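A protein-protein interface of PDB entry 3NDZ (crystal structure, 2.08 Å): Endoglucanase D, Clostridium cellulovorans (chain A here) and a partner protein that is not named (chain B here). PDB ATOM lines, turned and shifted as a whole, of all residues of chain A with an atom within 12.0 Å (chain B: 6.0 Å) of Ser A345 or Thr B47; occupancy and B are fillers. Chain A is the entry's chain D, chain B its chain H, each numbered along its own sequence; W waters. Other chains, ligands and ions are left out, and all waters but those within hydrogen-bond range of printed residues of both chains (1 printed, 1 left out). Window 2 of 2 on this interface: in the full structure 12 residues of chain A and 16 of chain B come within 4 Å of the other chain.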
ATOM      1  N   ASN A  17       7.399  16.881 -20.248  1.00  0.00           N
ATOM      2  CA  ASN A  17       6.451  16.389 -21.239  1.00  0.00           C
ATOM      3  C   ASN A  17       6.885  16.681 -22.691  1.00  0.00           C
ATOM      4  O   ASN A  17       6.775  15.816 -23.562  1.00  0.00           O
ATOM      5  CB  ASN A  17       5.056  16.967 -20.992  1.00  0.00           C
ATOM      6  CG  ASN A  17       4.418  16.467 -19.707  1.00  0.00           C
ATOM      7  OD1 ASN A  17       4.909  15.529 -19.046  1.00  0.00           O
ATOM      8  ND2 ASN A  17       3.304  17.095 -19.342  1.00  0.00           N
ATOM      9  N   GLU A  18       7.366  17.894 -22.955  1.00  0.00           N
ATOM     10  CA  GLU A  18       7.826  18.255 -24.300  1.00  0.00           C
ATOM     11  C   GLU A  18       9.122  17.536 -24.682  1.00  0.00           C
ATOM     12  O   GLU A  18       9.334  17.195 -25.849  1.00  0.00           O
ATOM     13  CB  GLU A  18       8.015  19.767 -24.425  1.00  0.00           C
ATOM     14  CG  GLU A  18       6.712  20.548 -24.355  1.00  0.00           C
ATOM     15  CD  GLU A  18       6.915  22.052 -24.487  1.00  0.00           C
ATOM     16  OE1 GLU A  18       8.054  22.477 -24.780  1.00  0.00           O
ATOM     17  OE2 GLU A  18       5.935  22.812 -24.294  1.00  0.00           O
ATOM     18  N   LYS A  20       9.700  14.602 -23.843  1.00  0.00           N
ATOM     19  CA  LYS A  20       8.961  13.449 -24.384  1.00  0.00           C
ATOM     20  C   LYS A  20       9.662  12.099 -24.268  1.00  0.00           C
ATOM     21  O   LYS A  20       9.215  11.228 -23.525  1.00  0.00           O
ATOM     22  CB  LYS A  20       8.526  13.716 -25.828  1.00  0.00           C
ATOM     23  CG  LYS A  20       7.641  12.629 -26.433  1.00  0.00           C
ATOM     24  CD  LYS A  20       7.203  13.021 -27.848  1.00  0.00           C
ATOM     25  CE  LYS A  20       6.128  12.077 -28.361  1.00  0.00           C
ATOM     26  NZ  LYS A  20       5.700  12.413 -29.743  1.00  0.00           N
ATOM     27  N   LYS A  52      16.156  12.128 -34.442  1.00  0.00           N
ATOM     28  CA  LYS A  52      14.912  12.887 -34.483  1.00  0.00           C
ATOM     29  C   LYS A  52      13.859  12.194 -35.342  1.00  0.00           C
ATOM     30  O   LYS A  52      12.686  12.112 -34.964  1.00  0.00           O
ATOM     31  CB  LYS A  52      15.161  14.302 -35.013  1.00  0.00           C
ATOM     32  CG  LYS A  52      13.884  15.115 -35.198  1.00  0.00           C
ATOM     33  CD  LYS A  52      13.273  15.536 -33.871  1.00  0.00           C
ATOM     34  CE  LYS A  52      11.907  16.194 -34.100  1.00  0.00           C
ATOM     35  NZ  LYS A  52      11.626  17.341 -33.188  1.00  0.00           N
ATOM     36  N   GLY A  55      11.675   9.585 -33.929  1.00  0.00           N
ATOM     37  CA  GLY A  55      10.688  10.049 -32.962  1.00  0.00           C
ATOM     38  C   GLY A  55      11.209  10.500 -31.598  1.00  0.00           C
ATOM     39  O   GLY A  55      10.424  10.809 -30.706  1.00  0.00           O
ATOM     40  N   ASN A  57      12.721  13.186 -29.116  1.00  0.00           N
ATOM     41  CA  ASN A  57      12.745  14.639 -29.087  1.00  0.00           C
ATOM     42  C   ASN A  57      13.816  15.219 -28.169  1.00  0.00           C
ATOM     43  O   ASN A  57      13.950  16.438 -28.065  1.00  0.00           O
ATOM     44  CB  ASN A  57      11.382  15.228 -28.729  1.00  0.00           C
ATOM     45  CG  ASN A  57      11.235  16.667 -29.217  1.00  0.00           C
ATOM     46  OD1 ASN A  57      11.664  16.992 -30.326  1.00  0.00           O
ATOM     47  ND2 ASN A  57      10.659  17.536 -28.386  1.00  0.00           N
ATOM     48  N   LYS A 296       5.639   6.838 -18.757  1.00  0.00           N
ATOM     49  CA  LYS A 296       4.898   8.001 -19.208  1.00  0.00           C
ATOM     50  C   LYS A 296       3.612   8.193 -18.398  1.00  0.00           C
ATOM     51  O   LYS A 296       3.179   9.324 -18.164  1.00  0.00           O
ATOM     52  CB  LYS A 296       4.591   7.881 -20.705  1.00  0.00           C
ATOM     53  CG  LYS A 296       4.035   9.149 -21.340  1.00  0.00           C
ATOM     54  CD  LYS A 296       4.948  10.372 -21.109  1.00  0.00           C
ATOM     55  CE  LYS A 296       6.343  10.197 -21.701  1.00  0.00           C
ATOM     56  NZ  LYS A 296       7.076  11.505 -21.749  1.00  0.00           N
ATOM     57  N   ILE A 338       9.453   3.839 -28.947  1.00  0.00           N
ATOM     58  CA  ILE A 338       8.785   5.043 -29.445  1.00  0.00           C
ATOM     59  C   ILE A 338       7.269   4.884 -29.421  1.00  0.00           C
ATOM     60  O   ILE A 338       6.544   5.815 -29.071  1.00  0.00           O
ATOM     61  CB  ILE A 338       9.247   5.422 -30.872  1.00  0.00           C
ATOM     62  CG1 ILE A 338      10.736   5.786 -30.866  1.00  0.00           C
ATOM     63  CG2 ILE A 338       8.425   6.587 -31.419  1.00  0.00           C
ATOM     64  CD1 ILE A 338      11.083   6.945 -29.931  1.00  0.00           C
ATOM     65  N   LYS A 339       6.792   3.696 -29.783  1.00  0.00           N
ATOM     66  CA  LYS A 339       5.358   3.462 -29.864  1.00  0.00           C
ATOM     67  C   LYS A 339       4.703   3.581 -28.491  1.00  0.00           C
ATOM     68  O   LYS A 339       3.632   4.165 -28.356  1.00  0.00           O
ATOM     69  CB  LYS A 339       5.067   2.086 -30.461  1.00  0.00           C
ATOM     70  CG  LYS A 339       3.596   1.843 -30.748  1.00  0.00           C
ATOM     71  CD  LYS A 339       3.319   0.341 -30.880  1.00  0.00           C
ATOM     72  CE  LYS A 339       1.851   0.059 -31.224  1.00  0.00           C
ATOM     73  NZ  LYS A 339       0.873   0.580 -30.212  1.00  0.00           N
ATOM     74  N   ILE A 341       5.551   5.448 -26.052  1.00  0.00           N
ATOM     75  CA  ILE A 341       5.553   6.829 -25.569  1.00  0.00           C
ATOM     76  C   ILE A 341       4.298   7.586 -26.016  1.00  0.00           C
ATOM     77  O   ILE A 341       3.792   8.450 -25.308  1.00  0.00           O
ATOM     78  CB  ILE A 341       6.797   7.591 -26.075  1.00  0.00           C
ATOM     79  CG1 ILE A 341       8.076   7.025 -25.446  1.00  0.00           C
ATOM     80  CG2 ILE A 341       6.660   9.088 -25.812  1.00  0.00           C
ATOM     81  CD1 ILE A 341       8.209   7.280 -23.942  1.00  0.00           C
ATOM     82  N   GLY A 342       3.797   7.254 -27.197  1.00  0.00           N
ATOM     83  CA  GLY A 342       2.639   7.933 -27.738  1.00  0.00           C
ATOM     84  C   GLY A 342       2.956   9.349 -28.176  1.00  0.00           C
ATOM     85  O   GLY A 342       4.107   9.693 -28.458  1.00  0.00           O
ATOM     86  N   GLY A 343       1.927  10.184 -28.218  1.00  0.00           N
ATOM     87  CA  GLY A 343       2.086  11.538 -28.694  1.00  0.00           C
ATOM     88  C   GLY A 343       0.785  12.300 -28.627  1.00  0.00           C
ATOM     89  O   GLY A 343      -0.230  11.767 -28.185  1.00  0.00           O
ATOM     90  N   SER A 344       0.825  13.551 -29.065  1.00  0.00           N
ATOM     91  CA  SER A 344      -0.321  14.445 -28.989  1.00  0.00           C
ATOM     92  C   SER A 344      -1.049  14.528 -30.328  1.00  0.00           C
ATOM     93  O   SER A 344      -2.057  15.220 -30.449  1.00  0.00           O
ATOM     94  CB  SER A 344       0.144  15.837 -28.593  1.00  0.00           C
ATOM     95  OG  SER A 344       0.866  16.415 -29.666  1.00  0.00           O
ATOM     96  N   SER A 345      -0.525  13.826 -31.329  1.00  0.00           N
ATOM     97  CA  SER A 345      -1.161  13.737 -32.641  1.00  0.00           C
ATOM     98  C   SER A 345      -0.804  12.430 -33.346  1.00  0.00           C
ATOM     99  O   SER A 345      -1.590  11.911 -34.142  1.00  0.00           O
ATOM    100  CB  SER A 345      -0.771  14.933 -33.515  1.00  0.00           C
ATOM    101  OG  SER A 345       0.445  15.521 -33.075  1.00  0.00           O
ATOM    102  N   THR B  45     -10.845  10.083 -36.484  1.00  0.00           N
ATOM    103  CA  THR B  45      -9.408  10.117 -36.223  1.00  0.00           C
ATOM    104  C   THR B  45      -9.074  11.307 -35.333  1.00  0.00           C
ATOM    105  O   THR B  45      -9.523  12.427 -35.588  1.00  0.00           O
ATOM    106  CB  THR B  45      -8.589  10.262 -37.519  1.00  0.00           C
ATOM    107  OG1 THR B  45      -8.945   9.218 -38.432  1.00  0.00           O
ATOM    108  CG2 THR B  45      -7.093  10.168 -37.211  1.00  0.00           C
ATOM    109  N   ILE B  46      -8.287  11.067 -34.290  1.00  0.00           N
ATOM    110  CA  ILE B  46      -7.832  12.153 -33.440  1.00  0.00           C
ATOM    111  C   ILE B  46      -6.705  12.895 -34.136  1.00  0.00           C
ATOM    112  O   ILE B  46      -5.704  12.292 -34.526  1.00  0.00           O
ATOM    113  CB  ILE B  46      -7.339  11.644 -32.081  1.00  0.00           C
ATOM    114  CG1 ILE B  46      -8.467  10.918 -31.351  1.00  0.00           C
ATOM    115  CG2 ILE B  46      -6.826  12.807 -31.252  1.00  0.00           C
ATOM    116  CD1 ILE B  46      -8.189  10.673 -29.894  1.00  0.00           C
ATOM    117  N   THR B  47      -6.871  14.201 -34.297  1.00  0.00           N
ATOM    118  CA  THR B  47      -5.866  15.014 -34.958  1.00  0.00           C
ATOM    119  C   THR B  47      -4.893  15.646 -33.966  1.00  0.00           C
ATOM    120  O   THR B  47      -3.695  15.701 -34.225  1.00  0.00           O
ATOM    121  CB  THR B  47      -6.507  16.100 -35.828  1.00  0.00           C
ATOM    122  OG1 THR B  47      -7.372  16.908 -35.023  1.00  0.00           O
ATOM    123  CG2 THR B  47      -7.332  15.452 -36.950  1.00  0.00           C
ATOM    124  N   ASN B  48      -5.406  16.141 -32.844  1.00  0.00           N
ATOM    125  CA  ASN B  48      -4.535  16.622 -31.779  1.00  0.00           C
ATOM    126  C   ASN B  48      -5.196  16.617 -30.396  1.00  0.00           C
ATOM    127  O   ASN B  48      -6.416  16.685 -30.280  1.00  0.00           O
ATOM    128  CB  ASN B  48      -3.933  17.987 -32.118  1.00  0.00           C
ATOM    129  CG  ASN B  48      -4.909  19.108 -31.949  1.00  0.00           C
ATOM    130  OD1 ASN B  48      -5.948  19.145 -32.609  1.00  0.00           O
ATOM    131  ND2 ASN B  48      -4.583  20.046 -31.062  1.00  0.00           N
ATOM    132  N   MET B  49      -4.372  16.500 -29.359  1.00  0.00           N
ATOM    133  CA  MET B  49      -4.846  16.317 -27.991  1.00  0.00           C
ATOM    134  C   MET B  49      -4.062  17.207 -27.020  1.00  0.00           C
ATOM    135  O   MET B  49      -2.854  17.390 -27.182  1.00  0.00           O
ATOM    136  CB  MET B  49      -4.686  14.847 -27.590  1.00  0.00           C
ATOM    137  CG  MET B  49      -5.182  14.511 -26.187  1.00  0.00           C
ATOM    138  SD  MET B  49      -5.082  12.761 -25.784  1.00  0.00           S
ATOM    139  CE  MET B  49      -6.364  12.073 -26.834  1.00  0.00           C
ATOM    140  N   PHE B  54      -1.761  10.244 -26.332  1.00  0.00           N
ATOM    141  CA  PHE B  54      -2.445   9.001 -26.649  1.00  0.00           C
ATOM    142  C   PHE B  54      -1.659   8.087 -27.576  1.00  0.00           C
ATOM    143  O   PHE B  54      -0.771   8.528 -28.311  1.00  0.00           O
ATOM    144  CB  PHE B  54      -3.814   9.288 -27.267  1.00  0.00           C
ATOM    145  CG  PHE B  54      -3.755   9.835 -28.674  1.00  0.00           C
ATOM    146  CD1 PHE B  54      -3.952   9.003 -29.767  1.00  0.00           C
ATOM    147  CD2 PHE B  54      -3.529  11.177 -28.900  1.00  0.00           C
ATOM    148  CE1 PHE B  54      -3.929   9.507 -31.066  1.00  0.00           C
ATOM    149  CE2 PHE B  54      -3.499  11.690 -30.196  1.00  0.00           C
ATOM    150  CZ  PHE B  54      -3.694  10.848 -31.279  1.00  0.00           C
ATOM    151  N   ASN B  84      -9.193  17.192 -30.665  1.00  0.00           N
ATOM    152  CA  ASN B  84      -9.943  17.393 -31.894  1.00  0.00           C
ATOM    153  C   ASN B  84      -9.957  16.097 -32.686  1.00  0.00           C
ATOM    154  O   ASN B  84      -8.995  15.324 -32.641  1.00  0.00           O
ATOM    155  CB  ASN B  84      -9.302  18.505 -32.735  1.00  0.00           C
ATOM    156  CG  ASN B  84      -9.438  19.874 -32.095  1.00  0.00           C
ATOM    157  OD1 ASN B  84     -10.435  20.166 -31.430  1.00  0.00           O
ATOM    158  ND2 ASN B  84      -8.436  20.724 -32.299  1.00  0.00           N
ATOM    159  N   ILE B  85     -11.056  15.851 -33.391  1.00  0.00           N
ATOM    160  CA  ILE B  85     -11.119  14.734 -34.314  1.00  0.00           C
ATOM    161  C   ILE B  85     -11.526  15.209 -35.696  1.00  0.00           C
ATOM    162  O   ILE B  85     -12.164  16.252 -35.844  1.00  0.00           O
ATOM    163  CB  ILE B  85     -12.157  13.689 -33.878  1.00  0.00           C
ATOM    164  CG1 ILE B  85     -13.556  14.300 -33.883  1.00  0.00           C
ATOM    165  CG2 ILE B  85     -11.806  13.099 -32.510  1.00  0.00           C
ATOM    166  CD1 ILE B  85     -14.635  13.296 -33.549  1.00  0.00           C
ATOM    167  N   ASN B  86     -11.132  14.441 -36.704  1.00  0.00           N
ATOM    168  CA  ASN B  86     -11.745  14.538 -38.017  1.00  0.00           C
ATOM    169  C   ASN B  86     -12.691  13.373 -38.132  1.00  0.00           C
ATOM    170  O   ASN B  86     -12.390  12.284 -37.649  1.00  0.00           O
ATOM    171  CB  ASN B  86     -10.698  14.465 -39.123  1.00  0.00           C
ATOM    172  CG  ASN B  86     -10.024  15.793 -39.363  1.00  0.00           C
ATOM    173  OD1 ASN B  86     -10.601  16.853 -39.106  1.00  0.00           O
ATOM    174  ND2 ASN B  86      -8.796  15.749 -39.857  1.00  0.00           N
HETATM  175  O   HOH W   1       0.159   9.161 -30.903  1.00  0.00           O
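The backbone carbonyl oxygen (O) of Gly A343 sits at hydrogen-bond distance from the backbone NH (N) of Phe B54.
N of Met B49 lies within hydrogen-bond range of O of Ser A344 (2.9 Å).
The backbone carbonyl oxygen of Gly A342 sits close to the side-chain amino group of Lys A20 (3.4 Å).
The backbone NH (N) of Thr B47 is in hydrogen-bond range of the backbone carbonyl oxygen (O) of Asn B84 (2.9 Å).
The backbone carbonyl oxygen (O) of Asn B48 sits at hydrogen-bond distance from the backbone NH (N) of Asn B84.
Gly A342 touches Phe B54.
Asn B48 touches Ser A344.
CE2 of Phe B54 touches C of Ser A344, 3.8 Å away.
O of Thr B47 touches CB of Ser A345, at 3.1 Å.
Ser A345 touches Phe B54 (O to CZ, 3.7 Å).
Lys A52 touches none of the printed residues of chain B.
Lys A296 touches none of the printed residues of chain B.
Of the printed residues of chain B, Gly A342 touches Phe B54.
Of the printed residues of chain B, Gly A343 touches Phe B54 (2.8 Å).
Of the printed residues of chain B, Ser A344 touches Asn B48 (3.1 Å), Met B49 (2.9 Å) and Phe B54 (3.8 Å).
Of chain B, only Thr B47 and Phe B54 come within 4 Å of Ser A345.
No residue of chain A comes within 4 Å of Ile B46.
Of chain A, only Ser A345 comes within 4 Å of Thr B47.
No residue of chain A comes within 4 Å of Ile B85.
The nearest residue of chain B that does not touch Ser A345 is Ile B46 (4.1 Å).
The nearest residue of chain A that does not touch Thr B47 is Ser A344 (4.1 Å).
Of the 14 printed residues of chain A, 4 touch a printed residue of chain B.
Printed residues of chain A that touch a printed residue of chain B: Gly A342, Gly A343, Ser A344 and Ser A345.
Hydrophobic or aromatic side chains of chain B within 4 Å of the printed part of chain A: Met B49 and Phe B54.
Among the printed residues, 7 pairs touch across the chains.
Water W1 bridges the backbone carbonyl oxygen (O) of Phe B54 (2.8 Å) and the backbone NH (N) of Gly A343 (3.4 Å).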
